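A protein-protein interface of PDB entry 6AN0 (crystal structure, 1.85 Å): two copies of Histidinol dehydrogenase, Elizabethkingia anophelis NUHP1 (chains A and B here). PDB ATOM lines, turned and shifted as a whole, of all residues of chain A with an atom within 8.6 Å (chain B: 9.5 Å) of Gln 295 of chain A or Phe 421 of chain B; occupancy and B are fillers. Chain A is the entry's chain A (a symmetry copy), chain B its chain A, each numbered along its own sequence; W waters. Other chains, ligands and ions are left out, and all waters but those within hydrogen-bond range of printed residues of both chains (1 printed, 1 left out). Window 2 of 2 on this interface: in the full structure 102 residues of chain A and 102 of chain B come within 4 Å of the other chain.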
ATOM      1  N   ALA A 258      -7.519  30.086 -27.039  1.00  0.00           N
ATOM      2  CA  ALA A 258      -6.950  29.236 -25.996  1.00  0.00           C
ATOM      3  C   ALA A 258      -6.045  30.029 -25.058  1.00  0.00           C
ATOM      4  O   ALA A 258      -6.045  29.795 -23.840  1.00  0.00           O
ATOM      5  CB  ALA A 258      -6.183  28.073 -26.633  1.00  0.00           C
ATOM      6  N   LEU A 261      -8.262  32.057 -22.742  1.00  0.00           N
ATOM      7  CA  LEU A 261      -8.905  31.217 -21.738  1.00  0.00           C
ATOM      8  C   LEU A 261      -7.899  30.678 -20.732  1.00  0.00           C
ATOM      9  O   LEU A 261      -8.257  30.440 -19.575  1.00  0.00           O
ATOM     10  CB  LEU A 261      -9.669  30.083 -22.415  1.00  0.00           C
ATOM     11  CG  LEU A 261     -10.942  30.568 -23.122  1.00  0.00           C
ATOM     12  CD1 LEU A 261     -11.549  29.482 -23.974  1.00  0.00           C
ATOM     13  CD2 LEU A 261     -11.957  31.049 -22.093  1.00  0.00           C
ATOM     14  N   SER A 262      -6.640  30.493 -21.142  1.00  0.00           N
ATOM     15  CA  SER A 262      -5.630  30.051 -20.186  1.00  0.00           C
ATOM     16  C   SER A 262      -5.429  31.090 -19.088  1.00  0.00           C
ATOM     17  O   SER A 262      -5.306  30.738 -17.910  1.00  0.00           O
ATOM     18  CB  SER A 262      -4.310  29.729 -20.899  1.00  0.00           C
ATOM     19  OG  SER A 262      -3.655  30.887 -21.385  1.00  0.00           O
ATOM     20  N   GLU A 265      -8.870  31.366 -16.722  1.00  0.00           N
ATOM     21  CA  GLU A 265      -9.157  30.316 -15.754  1.00  0.00           C
ATOM     22  C   GLU A 265      -8.362  30.465 -14.461  1.00  0.00           C
ATOM     23  O   GLU A 265      -8.608  29.699 -13.518  1.00  0.00           O
ATOM     24  CB  GLU A 265      -8.888  28.940 -16.374  1.00  0.00           C
ATOM     25  CG  GLU A 265      -7.424  28.530 -16.286  1.00  0.00           C
ATOM     26  CD  GLU A 265      -7.164  27.120 -16.799  1.00  0.00           C
ATOM     27  OE1 GLU A 265      -8.127  26.342 -16.949  1.00  0.00           O
ATOM     28  OE2 GLU A 265      -5.981  26.790 -17.053  1.00  0.00           O
ATOM     29  N   GLN A 288     -14.336  31.005 -31.163  1.00  0.00           N
ATOM     30  CA  GLN A 288     -13.482  29.979 -30.576  1.00  0.00           C
ATOM     31  C   GLN A 288     -13.530  30.029 -29.053  1.00  0.00           C
ATOM     32  O   GLN A 288     -13.522  28.984 -28.394  1.00  0.00           O
ATOM     33  CB  GLN A 288     -12.044  30.151 -31.072  1.00  0.00           C
ATOM     34  CG  GLN A 288     -11.794  29.623 -32.483  1.00  0.00           C
ATOM     35  CD  GLN A 288     -11.712  28.107 -32.548  1.00  0.00           C
ATOM     36  OE1 GLN A 288     -11.615  27.432 -31.525  1.00  0.00           O
ATOM     37  NE2 GLN A 288     -11.747  27.566 -33.762  1.00  0.00           N
ATOM     38  N   VAL A 289     -13.571  31.234 -28.479  1.00  0.00           N
ATOM     39  CA  VAL A 289     -13.668  31.361 -27.025  1.00  0.00           C
ATOM     40  C   VAL A 289     -14.936  30.692 -26.524  1.00  0.00           C
ATOM     41  O   VAL A 289     -14.911  29.922 -25.558  1.00  0.00           O
ATOM     42  CB  VAL A 289     -13.622  32.841 -26.605  1.00  0.00           C
ATOM     43  CG1 VAL A 289     -14.065  32.992 -25.138  1.00  0.00           C
ATOM     44  CG2 VAL A 289     -12.234  33.420 -26.812  1.00  0.00           C
ATOM     45  N   GLU A 290     -16.069  30.976 -27.180  1.00  0.00           N
ATOM     46  CA  GLU A 290     -17.335  30.406 -26.737  1.00  0.00           C
ATOM     47  C   GLU A 290     -17.303  28.886 -26.811  1.00  0.00           C
ATOM     48  O   GLU A 290     -17.730  28.200 -25.874  1.00  0.00           O
ATOM     49  CB  GLU A 290     -18.492  30.958 -27.580  1.00  0.00           C
ATOM     50  CG  GLU A 290     -18.790  32.435 -27.345  1.00  0.00           C
ATOM     51  CD  GLU A 290     -18.879  32.791 -25.865  1.00  0.00           C
ATOM     52  OE1 GLU A 290     -18.092  33.648 -25.408  1.00  0.00           O
ATOM     53  OE2 GLU A 290     -19.728  32.209 -25.157  1.00  0.00           O
ATOM     54  N   ASN A 291     -16.802  28.341 -27.927  1.00  0.00           N
ATOM     55  CA  ASN A 291     -16.767  26.890 -28.095  1.00  0.00           C
ATOM     56  C   ASN A 291     -15.806  26.234 -27.111  1.00  0.00           C
ATOM     57  O   ASN A 291     -16.144  25.218 -26.493  1.00  0.00           O
ATOM     58  CB  ASN A 291     -16.390  26.533 -29.529  1.00  0.00           C
ATOM     59  CG  ASN A 291     -17.510  26.801 -30.503  1.00  0.00           C
ATOM     60  OD1 ASN A 291     -18.662  26.985 -30.103  1.00  0.00           O
ATOM     61  ND2 ASN A 291     -17.186  26.816 -31.791  1.00  0.00           N
ATOM     62  N   GLN A 292     -14.608  26.798 -26.949  1.00  0.00           N
ATOM     63  CA  GLN A 292     -13.636  26.213 -26.031  1.00  0.00           C
ATOM     64  C   GLN A 292     -14.063  26.355 -24.577  1.00  0.00           C
ATOM     65  O   GLN A 292     -13.765  25.477 -23.760  1.00  0.00           O
ATOM     66  CB  GLN A 292     -12.257  26.852 -26.228  1.00  0.00           C
ATOM     67  CG  GLN A 292     -11.614  26.518 -27.558  1.00  0.00           C
ATOM     68  CD  GLN A 292     -10.232  27.122 -27.689  1.00  0.00           C
ATOM     69  OE1 GLN A 292      -9.499  27.218 -26.707  1.00  0.00           O
ATOM     70  NE2 GLN A 292      -9.871  27.538 -28.901  1.00  0.00           N
ATOM     71  N   LEU A 293     -14.755  27.445 -24.234  1.00  0.00           N
ATOM     72  CA  LEU A 293     -15.176  27.656 -22.852  1.00  0.00           C
ATOM     73  C   LEU A 293     -16.027  26.497 -22.343  1.00  0.00           C
ATOM     74  O   LEU A 293     -15.912  26.105 -21.177  1.00  0.00           O
ATOM     75  CB  LEU A 293     -15.943  28.973 -22.737  1.00  0.00           C
ATOM     76  CG  LEU A 293     -16.471  29.351 -21.350  1.00  0.00           C
ATOM     77  CD1 LEU A 293     -15.326  29.446 -20.360  1.00  0.00           C
ATOM     78  CD2 LEU A 293     -17.231  30.656 -21.413  1.00  0.00           C
ATOM     79  N   THR A 294     -16.875  25.928 -23.206  1.00  0.00           N
ATOM     80  CA  THR A 294     -17.763  24.848 -22.788  1.00  0.00           C
ATOM     81  C   THR A 294     -17.004  23.635 -22.262  1.00  0.00           C
ATOM     82  O   THR A 294     -17.577  22.835 -21.515  1.00  0.00           O
ATOM     83  CB  THR A 294     -18.669  24.409 -23.948  1.00  0.00           C
ATOM     84  OG1 THR A 294     -17.867  23.939 -25.039  1.00  0.00           O
ATOM     85  CG2 THR A 294     -19.537  25.561 -24.428  1.00  0.00           C
ATOM     86  N   GLN A 295     -15.735  23.481 -22.624  1.00  0.00           N
ATOM     87  CA  GLN A 295     -14.968  22.302 -22.260  1.00  0.00           C
ATOM     88  C   GLN A 295     -14.104  22.498 -21.017  1.00  0.00           C
ATOM     89  O   GLN A 295     -13.417  21.557 -20.607  1.00  0.00           O
ATOM     90  CB  GLN A 295     -14.090  21.877 -23.442  1.00  0.00           C
ATOM     91  CG  GLN A 295     -14.873  21.689 -24.737  1.00  0.00           C
ATOM     92  CD  GLN A 295     -15.957  20.625 -24.619  1.00  0.00           C
ATOM     93  OE1 GLN A 295     -15.677  19.472 -24.301  1.00  0.00           O
ATOM     94  NE2 GLN A 295     -17.201  21.014 -24.878  1.00  0.00           N
ATOM     95  N   LEU A 296     -14.122  23.682 -20.403  1.00  0.00           N
ATOM     96  CA  LEU A 296     -13.216  23.970 -19.291  1.00  0.00           C
ATOM     97  C   LEU A 296     -13.824  23.486 -17.984  1.00  0.00           C
ATOM     98  O   LEU A 296     -14.930  23.916 -17.636  1.00  0.00           O
ATOM     99  CB  LEU A 296     -12.939  25.460 -19.188  1.00  0.00           C
ATOM    100  CG  LEU A 296     -12.156  26.184 -20.284  1.00  0.00           C
ATOM    101  CD1 LEU A 296     -11.678  27.525 -19.752  1.00  0.00           C
ATOM    102  CD2 LEU A 296     -11.005  25.344 -20.781  1.00  0.00           C
ATOM    103  N   PRO A 297     -13.147  22.627 -17.221  1.00  0.00           N
ATOM    104  CA  PRO A 297     -13.633  22.339 -15.864  1.00  0.00           C
ATOM    105  C   PRO A 297     -13.789  23.597 -15.025  1.00  0.00           C
ATOM    106  O   PRO A 297     -14.706  23.672 -14.199  1.00  0.00           O
ATOM    107  CB  PRO A 297     -12.555  21.401 -15.301  1.00  0.00           C
ATOM    108  CG  PRO A 297     -11.940  20.780 -16.491  1.00  0.00           C
ATOM    109  CD  PRO A 297     -11.936  21.854 -17.546  1.00  0.00           C
ATOM    110  N   ARG A 298     -12.937  24.602 -15.241  1.00  0.00           N
ATOM    111  CA  ARG A 298     -13.012  25.877 -14.539  1.00  0.00           C
ATOM    112  C   ARG A 298     -13.808  26.922 -15.311  1.00  0.00           C
ATOM    113  O   ARG A 298     -13.498  28.119 -15.218  1.00  0.00           O
ATOM    114  CB  ARG A 298     -11.602  26.394 -14.249  1.00  0.00           C
ATOM    115  CG  ARG A 298     -10.787  25.456 -13.364  1.00  0.00           C
ATOM    116  CD  ARG A 298      -9.323  25.828 -13.344  1.00  0.00           C
ATOM    117  NE  ARG A 298      -9.080  27.145 -12.763  1.00  0.00           N
ATOM    118  CZ  ARG A 298      -8.861  27.355 -11.469  1.00  0.00           C
ATOM    119  NH1 ARG A 298      -8.877  26.334 -10.618  1.00  0.00           N
ATOM    120  NH2 ARG A 298      -8.636  28.588 -11.022  1.00  0.00           N
ATOM    121  N   LYS A 299     -14.827  26.503 -16.069  1.00  0.00           N
ATOM    122  CA  LYS A 299     -15.520  27.446 -16.943  1.00  0.00           C
ATOM    123  C   LYS A 299     -16.212  28.542 -16.145  1.00  0.00           C
ATOM    124  O   LYS A 299     -16.331  29.675 -16.625  1.00  0.00           O
ATOM    125  CB  LYS A 299     -16.530  26.710 -17.829  1.00  0.00           C
ATOM    126  CG  LYS A 299     -17.684  26.074 -17.067  1.00  0.00           C
ATOM    127  CD  LYS A 299     -18.672  25.394 -18.004  1.00  0.00           C
ATOM    128  CE  LYS A 299     -18.080  24.134 -18.623  1.00  0.00           C
ATOM    129  NZ  LYS A 299     -19.080  23.452 -19.490  1.00  0.00           N
ATOM    130  N   SER A 361       1.343  29.693 -21.525  1.00  0.00           N
ATOM    131  CA  SER A 361       1.592  28.508 -20.706  1.00  0.00           C
ATOM    132  C   SER A 361       3.059  28.108 -20.717  1.00  0.00           C
ATOM    133  O   SER A 361       3.582  27.640 -19.700  1.00  0.00           O
ATOM    134  CB  SER A 361       0.732  27.335 -21.188  1.00  0.00           C
ATOM    135  OG  SER A 361      -0.633  27.645 -21.044  1.00  0.00           O
ATOM    136  N   TYR A 365       5.468  27.862 -17.276  1.00  0.00           N
ATOM    137  CA  TYR A 365       5.983  26.589 -16.791  1.00  0.00           C
ATOM    138  C   TYR A 365       7.436  26.323 -17.151  1.00  0.00           C
ATOM    139  O   TYR A 365       8.212  25.925 -16.273  1.00  0.00           O
ATOM    140  CB  TYR A 365       5.125  25.429 -17.314  1.00  0.00           C
ATOM    141  CG  TYR A 365       3.783  25.324 -16.641  1.00  0.00           C
ATOM    142  CD1 TYR A 365       3.679  24.878 -15.327  1.00  0.00           C
ATOM    143  CD2 TYR A 365       2.618  25.668 -17.316  1.00  0.00           C
ATOM    144  CE1 TYR A 365       2.449  24.777 -14.706  1.00  0.00           C
ATOM    145  CE2 TYR A 365       1.388  25.570 -16.707  1.00  0.00           C
ATOM    146  CZ  TYR A 365       1.307  25.134 -15.400  1.00  0.00           C
ATOM    147  OH  TYR A 365       0.075  25.044 -14.795  1.00  0.00           O
ATOM    148  N   ILE B 411       4.994  20.686 -20.441  1.00  0.00           N
ATOM    149  CA  ILE B 411       4.066  21.715 -19.963  1.00  0.00           C
ATOM    150  C   ILE B 411       2.686  21.114 -19.704  1.00  0.00           C
ATOM    151  O   ILE B 411       2.054  21.377 -18.671  1.00  0.00           O
ATOM    152  CB  ILE B 411       3.983  22.867 -20.978  1.00  0.00           C
ATOM    153  CG1 ILE B 411       5.340  23.550 -21.129  1.00  0.00           C
ATOM    154  CG2 ILE B 411       2.891  23.883 -20.562  1.00  0.00           C
ATOM    155  CD1 ILE B 411       5.438  24.406 -22.361  1.00  0.00           C
ATOM    156  N   GLU B 412       2.187  20.317 -20.652  1.00  0.00           N
ATOM    157  CA  GLU B 412       0.892  19.664 -20.472  1.00  0.00           C
ATOM    158  C   GLU B 412       0.832  18.863 -19.172  1.00  0.00           C
ATOM    159  O   GLU B 412      -0.176  18.908 -18.454  1.00  0.00           O
ATOM    160  CB  GLU B 412       0.589  18.751 -21.665  1.00  0.00           C
ATOM    161  CG  GLU B 412       0.335  19.462 -22.997  1.00  0.00           C
ATOM    162  CD  GLU B 412      -0.022  18.480 -24.113  1.00  0.00           C
ATOM    163  OE1 GLU B 412      -0.852  18.819 -24.982  1.00  0.00           O
ATOM    164  OE2 GLU B 412       0.525  17.360 -24.116  1.00  0.00           O
ATOM    165  N   MET B 414       2.610  19.313 -16.406  1.00  0.00           N
ATOM    166  CA  MET B 414       2.624  20.204 -15.249  1.00  0.00           C
ATOM    167  C   MET B 414       1.297  20.943 -15.109  1.00  0.00           C
ATOM    168  O   MET B 414       0.794  21.123 -13.994  1.00  0.00           O
ATOM    169  CB  MET B 414       3.795  21.184 -15.355  1.00  0.00           C
ATOM    170  CG  MET B 414       5.128  20.544 -14.948  1.00  0.00           C
ATOM    171  SD  MET B 414       6.524  21.619 -15.255  1.00  0.00           S
ATOM    172  CE  MET B 414       6.490  21.791 -17.027  1.00  0.00           C
ATOM    173  N   ALA B 415       0.707  21.358 -16.229  1.00  0.00           N
ATOM    174  CA  ALA B 415      -0.600  22.008 -16.169  1.00  0.00           C
ATOM    175  C   ALA B 415      -1.655  21.053 -15.620  1.00  0.00           C
ATOM    176  O   ALA B 415      -2.488  21.449 -14.800  1.00  0.00           O
ATOM    177  CB  ALA B 415      -0.996  22.517 -17.555  1.00  0.00           C
ATOM    178  N   GLU B 416      -1.629  19.789 -16.061  1.00  0.00           N
ATOM    179  CA  GLU B 416      -2.505  18.764 -15.496  1.00  0.00           C
ATOM    180  C   GLU B 416      -2.355  18.671 -13.981  1.00  0.00           C
ATOM    181  O   GLU B 416      -3.350  18.611 -13.249  1.00  0.00           O
ATOM    182  CB  GLU B 416      -2.203  17.399 -16.119  1.00  0.00           C
ATOM    183  CG  GLU B 416      -2.713  17.188 -17.526  1.00  0.00           C
ATOM    184  CD  GLU B 416      -2.221  15.869 -18.108  1.00  0.00           C
ATOM    185  OE1 GLU B 416      -2.070  15.769 -19.344  1.00  0.00           O
ATOM    186  OE2 GLU B 416      -1.973  14.936 -17.317  1.00  0.00           O
ATOM    187  N   ALA B 417      -1.107  18.617 -13.497  1.00  0.00           N
ATOM    188  CA  ALA B 417      -0.864  18.500 -12.060  1.00  0.00           C
ATOM    189  C   ALA B 417      -1.344  19.731 -11.294  1.00  0.00           C
ATOM    190  O   ALA B 417      -1.766  19.614 -10.136  1.00  0.00           O
ATOM    191  CB  ALA B 417       0.621  18.256 -11.793  1.00  0.00           C
ATOM    192  N   GLU B 418      -1.279  20.914 -11.906  1.00  0.00           N
ATOM    193  CA  GLU B 418      -1.847  22.113 -11.300  1.00  0.00           C
ATOM    194  C   GLU B 418      -3.344  22.249 -11.560  1.00  0.00           C
ATOM    195  O   GLU B 418      -3.935  23.263 -11.169  1.00  0.00           O
ATOM    196  CB  GLU B 418      -1.106  23.365 -11.799  1.00  0.00           C
ATOM    197  CG  GLU B 418       0.384  23.412 -11.387  1.00  0.00           C
ATOM    198  CD  GLU B 418       1.029  24.792 -11.538  1.00  0.00           C
ATOM    199  OE1 GLU B 418       0.480  25.643 -12.271  1.00  0.00           O
ATOM    200  OE2 GLU B 418       2.092  25.031 -10.911  1.00  0.00           O
ATOM    201  N   GLU B 419      -3.960  21.254 -12.205  1.00  0.00           N
ATOM    202  CA  GLU B 419      -5.390  21.247 -12.531  1.00  0.00           C
ATOM    203  C   GLU B 419      -5.803  22.509 -13.287  1.00  0.00           C
ATOM    204  O   GLU B 419      -6.809  23.145 -12.975  1.00  0.00           O
ATOM    205  CB  GLU B 419      -6.237  21.056 -11.271  1.00  0.00           C
ATOM    206  CG  GLU B 419      -6.224  19.624 -10.748  1.00  0.00           C
ATOM    207  CD  GLU B 419      -6.814  19.483  -9.351  1.00  0.00           C
ATOM    208  OE1 GLU B 419      -6.690  18.386  -8.767  1.00  0.00           O
ATOM    209  OE2 GLU B 419      -7.396  20.461  -8.834  1.00  0.00           O
ATOM    210  N   LEU B 420      -5.015  22.867 -14.303  1.00  0.00           N
ATOM    211  CA  LEU B 420      -5.264  24.050 -15.134  1.00  0.00           C
ATOM    212  C   LEU B 420      -5.451  23.593 -16.581  1.00  0.00           C
ATOM    213  O   LEU B 420      -4.526  23.641 -17.393  1.00  0.00           O
ATOM    214  CB  LEU B 420      -4.141  25.055 -14.998  1.00  0.00           C
ATOM    215  CG  LEU B 420      -4.037  25.715 -13.617  1.00  0.00           C
ATOM    216  CD1 LEU B 420      -2.868  26.703 -13.551  1.00  0.00           C
ATOM    217  CD2 LEU B 420      -5.341  26.411 -13.259  1.00  0.00           C
ATOM    218  N   PHE B 421      -6.672  23.165 -16.899  1.00  0.00           N
ATOM    219  CA  PHE B 421      -6.934  22.532 -18.189  1.00  0.00           C
ATOM    220  C   PHE B 421      -6.752  23.496 -19.359  1.00  0.00           C
ATOM    221  O   PHE B 421      -6.291  23.089 -20.432  1.00  0.00           O
ATOM    222  CB  PHE B 421      -8.344  21.943 -18.216  1.00  0.00           C
ATOM    223  CG  PHE B 421      -8.738  21.414 -19.563  1.00  0.00           C
ATOM    224  CD1 PHE B 421      -8.295  20.170 -19.987  1.00  0.00           C
ATOM    225  CD2 PHE B 421      -9.519  22.173 -20.422  1.00  0.00           C
ATOM    226  CE1 PHE B 421      -8.640  19.686 -21.233  1.00  0.00           C
ATOM    227  CE2 PHE B 421      -9.871  21.692 -21.667  1.00  0.00           C
ATOM    228  CZ  PHE B 421      -9.430  20.449 -22.073  1.00  0.00           C
ATOM    229  N   ALA B 422      -7.143  24.765 -19.198  1.00  0.00           N
ATOM    230  CA  ALA B 422      -6.949  25.712 -20.294  1.00  0.00           C
ATOM    231  C   ALA B 422      -5.472  25.946 -20.568  1.00  0.00           C
ATOM    232  O   ALA B 422      -5.086  26.159 -21.726  1.00  0.00           O
ATOM    233  CB  ALA B 422      -7.648  27.040 -20.004  1.00  0.00           C
ATOM    234  N   HIS B 423      -4.638  25.919 -19.520  1.00  0.00           N
ATOM    235  CA  HIS B 423      -3.193  26.005 -19.721  1.00  0.00           C
ATOM    236  C   HIS B 423      -2.695  24.838 -20.561  1.00  0.00           C
ATOM    237  O   HIS B 423      -1.884  25.017 -21.476  1.00  0.00           O
ATOM    238  CB  HIS B 423      -2.469  26.032 -18.373  1.00  0.00           C
ATOM    239  CG  HIS B 423      -2.459  27.373 -17.709  1.00  0.00           C
ATOM    240  ND1 HIS B 423      -3.594  27.953 -17.180  1.00  0.00           N
ATOM    241  CD2 HIS B 423      -1.447  28.245 -17.478  1.00  0.00           C
ATOM    242  CE1 HIS B 423      -3.280  29.122 -16.648  1.00  0.00           C
ATOM    243  NE2 HIS B 423      -1.984  29.323 -16.818  1.00  0.00           N
ATOM    244  N   LYS B 424      -3.153  23.627 -20.240  1.00  0.00           N
ATOM    245  CA  LYS B 424      -2.799  22.455 -21.035  1.00  0.00           C
ATOM    246  C   LYS B 424      -3.319  22.578 -22.464  1.00  0.00           C
ATOM    247  O   LYS B 424      -2.614  22.243 -23.422  1.00  0.00           O
ATOM    248  CB  LYS B 424      -3.361  21.191 -20.385  1.00  0.00           C
ATOM    249  CG  LYS B 424      -3.308  19.967 -21.284  1.00  0.00           C
ATOM    250  CD  LYS B 424      -3.975  18.759 -20.634  1.00  0.00           C
ATOM    251  CE  LYS B 424      -4.129  17.619 -21.630  1.00  0.00           C
ATOM    252  NZ  LYS B 424      -4.616  16.373 -20.963  1.00  0.00           N
ATOM    253  N   HIS B 425      -4.554  23.056 -22.626  1.00  0.00           N
ATOM    254  CA  HIS B 425      -5.158  23.096 -23.956  1.00  0.00           C
ATOM    255  C   HIS B 425      -4.460  24.101 -24.869  1.00  0.00           C
ATOM    256  O   HIS B 425      -4.410  23.891 -26.084  1.00  0.00           O
ATOM    257  CB  HIS B 425      -6.651  23.420 -23.848  1.00  0.00           C
ATOM    258  CG  HIS B 425      -7.409  23.205 -25.124  1.00  0.00           C
ATOM    259  ND1 HIS B 425      -7.599  21.956 -25.678  1.00  0.00           N
ATOM    260  CD2 HIS B 425      -8.011  24.083 -25.961  1.00  0.00           C
ATOM    261  CE1 HIS B 425      -8.296  22.072 -26.795  1.00  0.00           C
ATOM    262  NE2 HIS B 425      -8.560  23.352 -26.989  1.00  0.00           N
ATOM    263  N   ALA B 426      -3.919  25.190 -24.310  1.00  0.00           N
ATOM    264  CA  ALA B 426      -3.220  26.175 -25.135  1.00  0.00           C
ATOM    265  C   ALA B 426      -1.985  25.573 -25.802  1.00  0.00           C
ATOM    266  O   ALA B 426      -1.608  25.991 -26.905  1.00  0.00           O
ATOM    267  CB  ALA B 426      -2.827  27.388 -24.289  1.00  0.00           C
ATOM    268  N   VAL B 427      -1.343  24.605 -25.144  1.00  0.00           N
ATOM    269  CA  VAL B 427      -0.275  23.834 -25.781  1.00  0.00           C
ATOM    270  C   VAL B 427      -0.858  22.820 -26.761  1.00  0.00           C
ATOM    271  O   VAL B 427      -0.401  22.700 -27.904  1.00  0.00           O
ATOM    272  CB  VAL B 427       0.593  23.138 -24.711  1.00  0.00           C
ATOM    273  CG1 VAL B 427       1.622  22.187 -25.372  1.00  0.00           C
ATOM    274  CG2 VAL B 427       1.284  24.151 -23.820  1.00  0.00           C
ATOM    275  N   SER B 428      -1.896  22.098 -26.328  1.00  0.00           N
ATOM    276  CA  SER B 428      -2.446  21.014 -27.137  1.00  0.00           C
ATOM    277  C   SER B 428      -2.858  21.485 -28.529  1.00  0.00           C
ATOM    278  O   SER B 428      -2.617  20.783 -29.518  1.00  0.00           O
ATOM    279  CB  SER B 428      -3.631  20.375 -26.412  1.00  0.00           C
ATOM    280  OG  SER B 428      -3.253  19.978 -25.103  1.00  0.00           O
ATOM    281  N   VAL B 429      -3.466  22.673 -28.639  1.00  0.00           N
ATOM    282  CA  VAL B 429      -3.919  23.115 -29.958  1.00  0.00           C
ATOM    283  C   VAL B 429      -2.745  23.377 -30.898  1.00  0.00           C
ATOM    284  O   VAL B 429      -2.851  23.146 -32.110  1.00  0.00           O
ATOM    285  CB  VAL B 429      -4.843  24.342 -29.849  1.00  0.00           C
ATOM    286  CG1 VAL B 429      -6.105  23.972 -29.094  1.00  0.00           C
ATOM    287  CG2 VAL B 429      -4.123  25.533 -29.195  1.00  0.00           C
ATOM    288  N   LYS B 432      -1.443  19.721 -31.969  1.00  0.00           N
ATOM    289  CA  LYS B 432      -2.333  19.061 -32.920  1.00  0.00           C
ATOM    290  C   LYS B 432      -2.276  19.730 -34.288  1.00  0.00           C
ATOM    291  O   LYS B 432      -2.410  19.055 -35.314  1.00  0.00           O
ATOM    292  CB  LYS B 432      -3.768  19.047 -32.389  1.00  0.00           C
ATOM    293  CG  LYS B 432      -3.956  18.263 -31.092  1.00  0.00           C
ATOM    294  CD  LYS B 432      -5.437  17.997 -30.814  1.00  0.00           C
ATOM    295  CE  LYS B 432      -5.803  18.196 -29.339  1.00  0.00           C
ATOM    296  NZ  LYS B 432      -6.314  19.574 -29.028  1.00  0.00           N
HETATM  297  O   HOH W   1      -6.881  27.091 -23.440  1.00  0.00           O
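The backbone carbonyl oxygen (O) of Ala 415 of chain B is in hydrogen-bond range of the backbone NH (N) of Leu 420 of chain B. The backbone carbonyl oxygen (O) of Glu 265 of chain A lies within hydrogen-bond range of the guanidinium group (NE) of Arg 298 of chain A, 2.7 Å away. The side-chain amide oxygen of Gln 288 of chain A lies within hydrogen-bond range of the side-chain amide nitrogen of Gln 292 of chain A, 3.2 Å away. OG1 of Thr 294 of chain A is in hydrogen-bond range of NE2 of Gln 295 of chain A, at 3.0 Å.
Of the printed residues of chain B, Glu 265 of chain A touches Leu 420 (3.3 Å), Phe 421 (3.5 Å), Ala 422 (2.9 Å) and His 423 (2.7 Å). Of the printed residues of chain B, Gln 292 of chain A touches His 425. No residue of chain B comes within 4 Å of Thr 294 of chain A. Of chain B, only Phe 421 comes within 4 Å of Gln 295 of chain A. Of chain A, only Glu 265 (3.5 Å), Gln 295 (3.7 Å), Leu 296 (3.5 Å) and Pro 297 (3.7 Å) come within 4 Å of Phe 421 of chain B. Of the printed residues of chain A, His 425 of chain B touches Gln 292. Lys 432 of chain B touches none of the printed residues of chain A. The nearest residue of chain B that does not touch Gln 295 of chain A is His 425 of chain B (6.7 Å). The nearest residue of chain A that does not touch Phe 421 of chain B is Arg 298 of chain A (5.2 Å). The nearest printed residue of chain A that does not touch Glu 419 of chain B is Glu 265 of chain A (5.3 Å).
No position is printed for both chains. Of the 24 pairs that touch across the chains among the printed residues, none has its exchanged pair printed and touching as well.
Water W1 lies within hydrogen-bond range of the backbone carbonyl oxygen of Ala 422 of chain B (2.7 Å) and the backbone carbonyl oxygen of Ala 258 of chain A (2.9 Å).
Of the 19 printed residues of chain B, 11 touch a printed residue of chain A. Hydrophobic or aromatic side chains of chain B within 4 Å of the printed part of chain A: Ile 411, Met 414, Ala 415, Leu 420, Phe 421, Ala 422, His 423, His 425 and Ala 426. Of the 18 printed residues of chain A, 11 touch a printed residue of chain B.
The side-chain hydroxyl (OH) of Tyr 365 of chain A is in hydrogen-bond range of the side-chain carboxylate (OE1) of Glu 418 of chain B, 2.6 Å away. The side-chain carboxylate (OE1) of Glu 265 of chain A is in hydrogen-bond range of the backbone NH (N) of Phe 421 of chain B (3.5 Å). The side-chain carboxylate (OE1) of Glu 265 of chain A is in hydrogen-bond range of the backbone NH (N) of Ala 422 of chain B. ND1 of His 423 of chain B lies close to O of Ser 262 of chain A, 3.3 Å away. A ring nitrogen (ND1) of His 423 of chain B lies within hydrogen-bond range of the side-chain carboxylate (OE2) of Glu 265 of chain A. The side-chain hydroxyl (OG) of Ser 361 of chain A is in hydrogen-bond range of the backbone carbonyl oxygen (O) of His 423 of chain B, 2.9 Å away. O of Leu 420 of chain B lies close to OE2 of Glu 265 of chain A, at 3.5 Å.
CB of Ala 258 of chain A touches CA of Ala 426 of chain B, 3.8 Å away. Gln 292 of chain A touches His 425 of chain B (OE1 to CD2, 3.5 Å). Phe 421 of chain B touches Leu 296 of chain A. Ala 422 of chain B touches Leu 296 of chain A (CB to CD2, 3.8 Å). Arg 298 of chain A touches Glu 419 of chain B. Arg 298 of chain A touches Leu 420 of chain B. CG2 of Ile 411 of chain B touches O of Ser 361 of chain A (3.9 Å). OG of Ser 361 of chain A touches CB of Ala 426 of chain B, 3.9 Å away. Tyr 365 of chain A touches Ile 411 of chain B (CD2 to CG2, 3.7 Å). OH of Tyr 365 of chain A touches CD1 of Leu 420 of chain B (3.6 Å).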
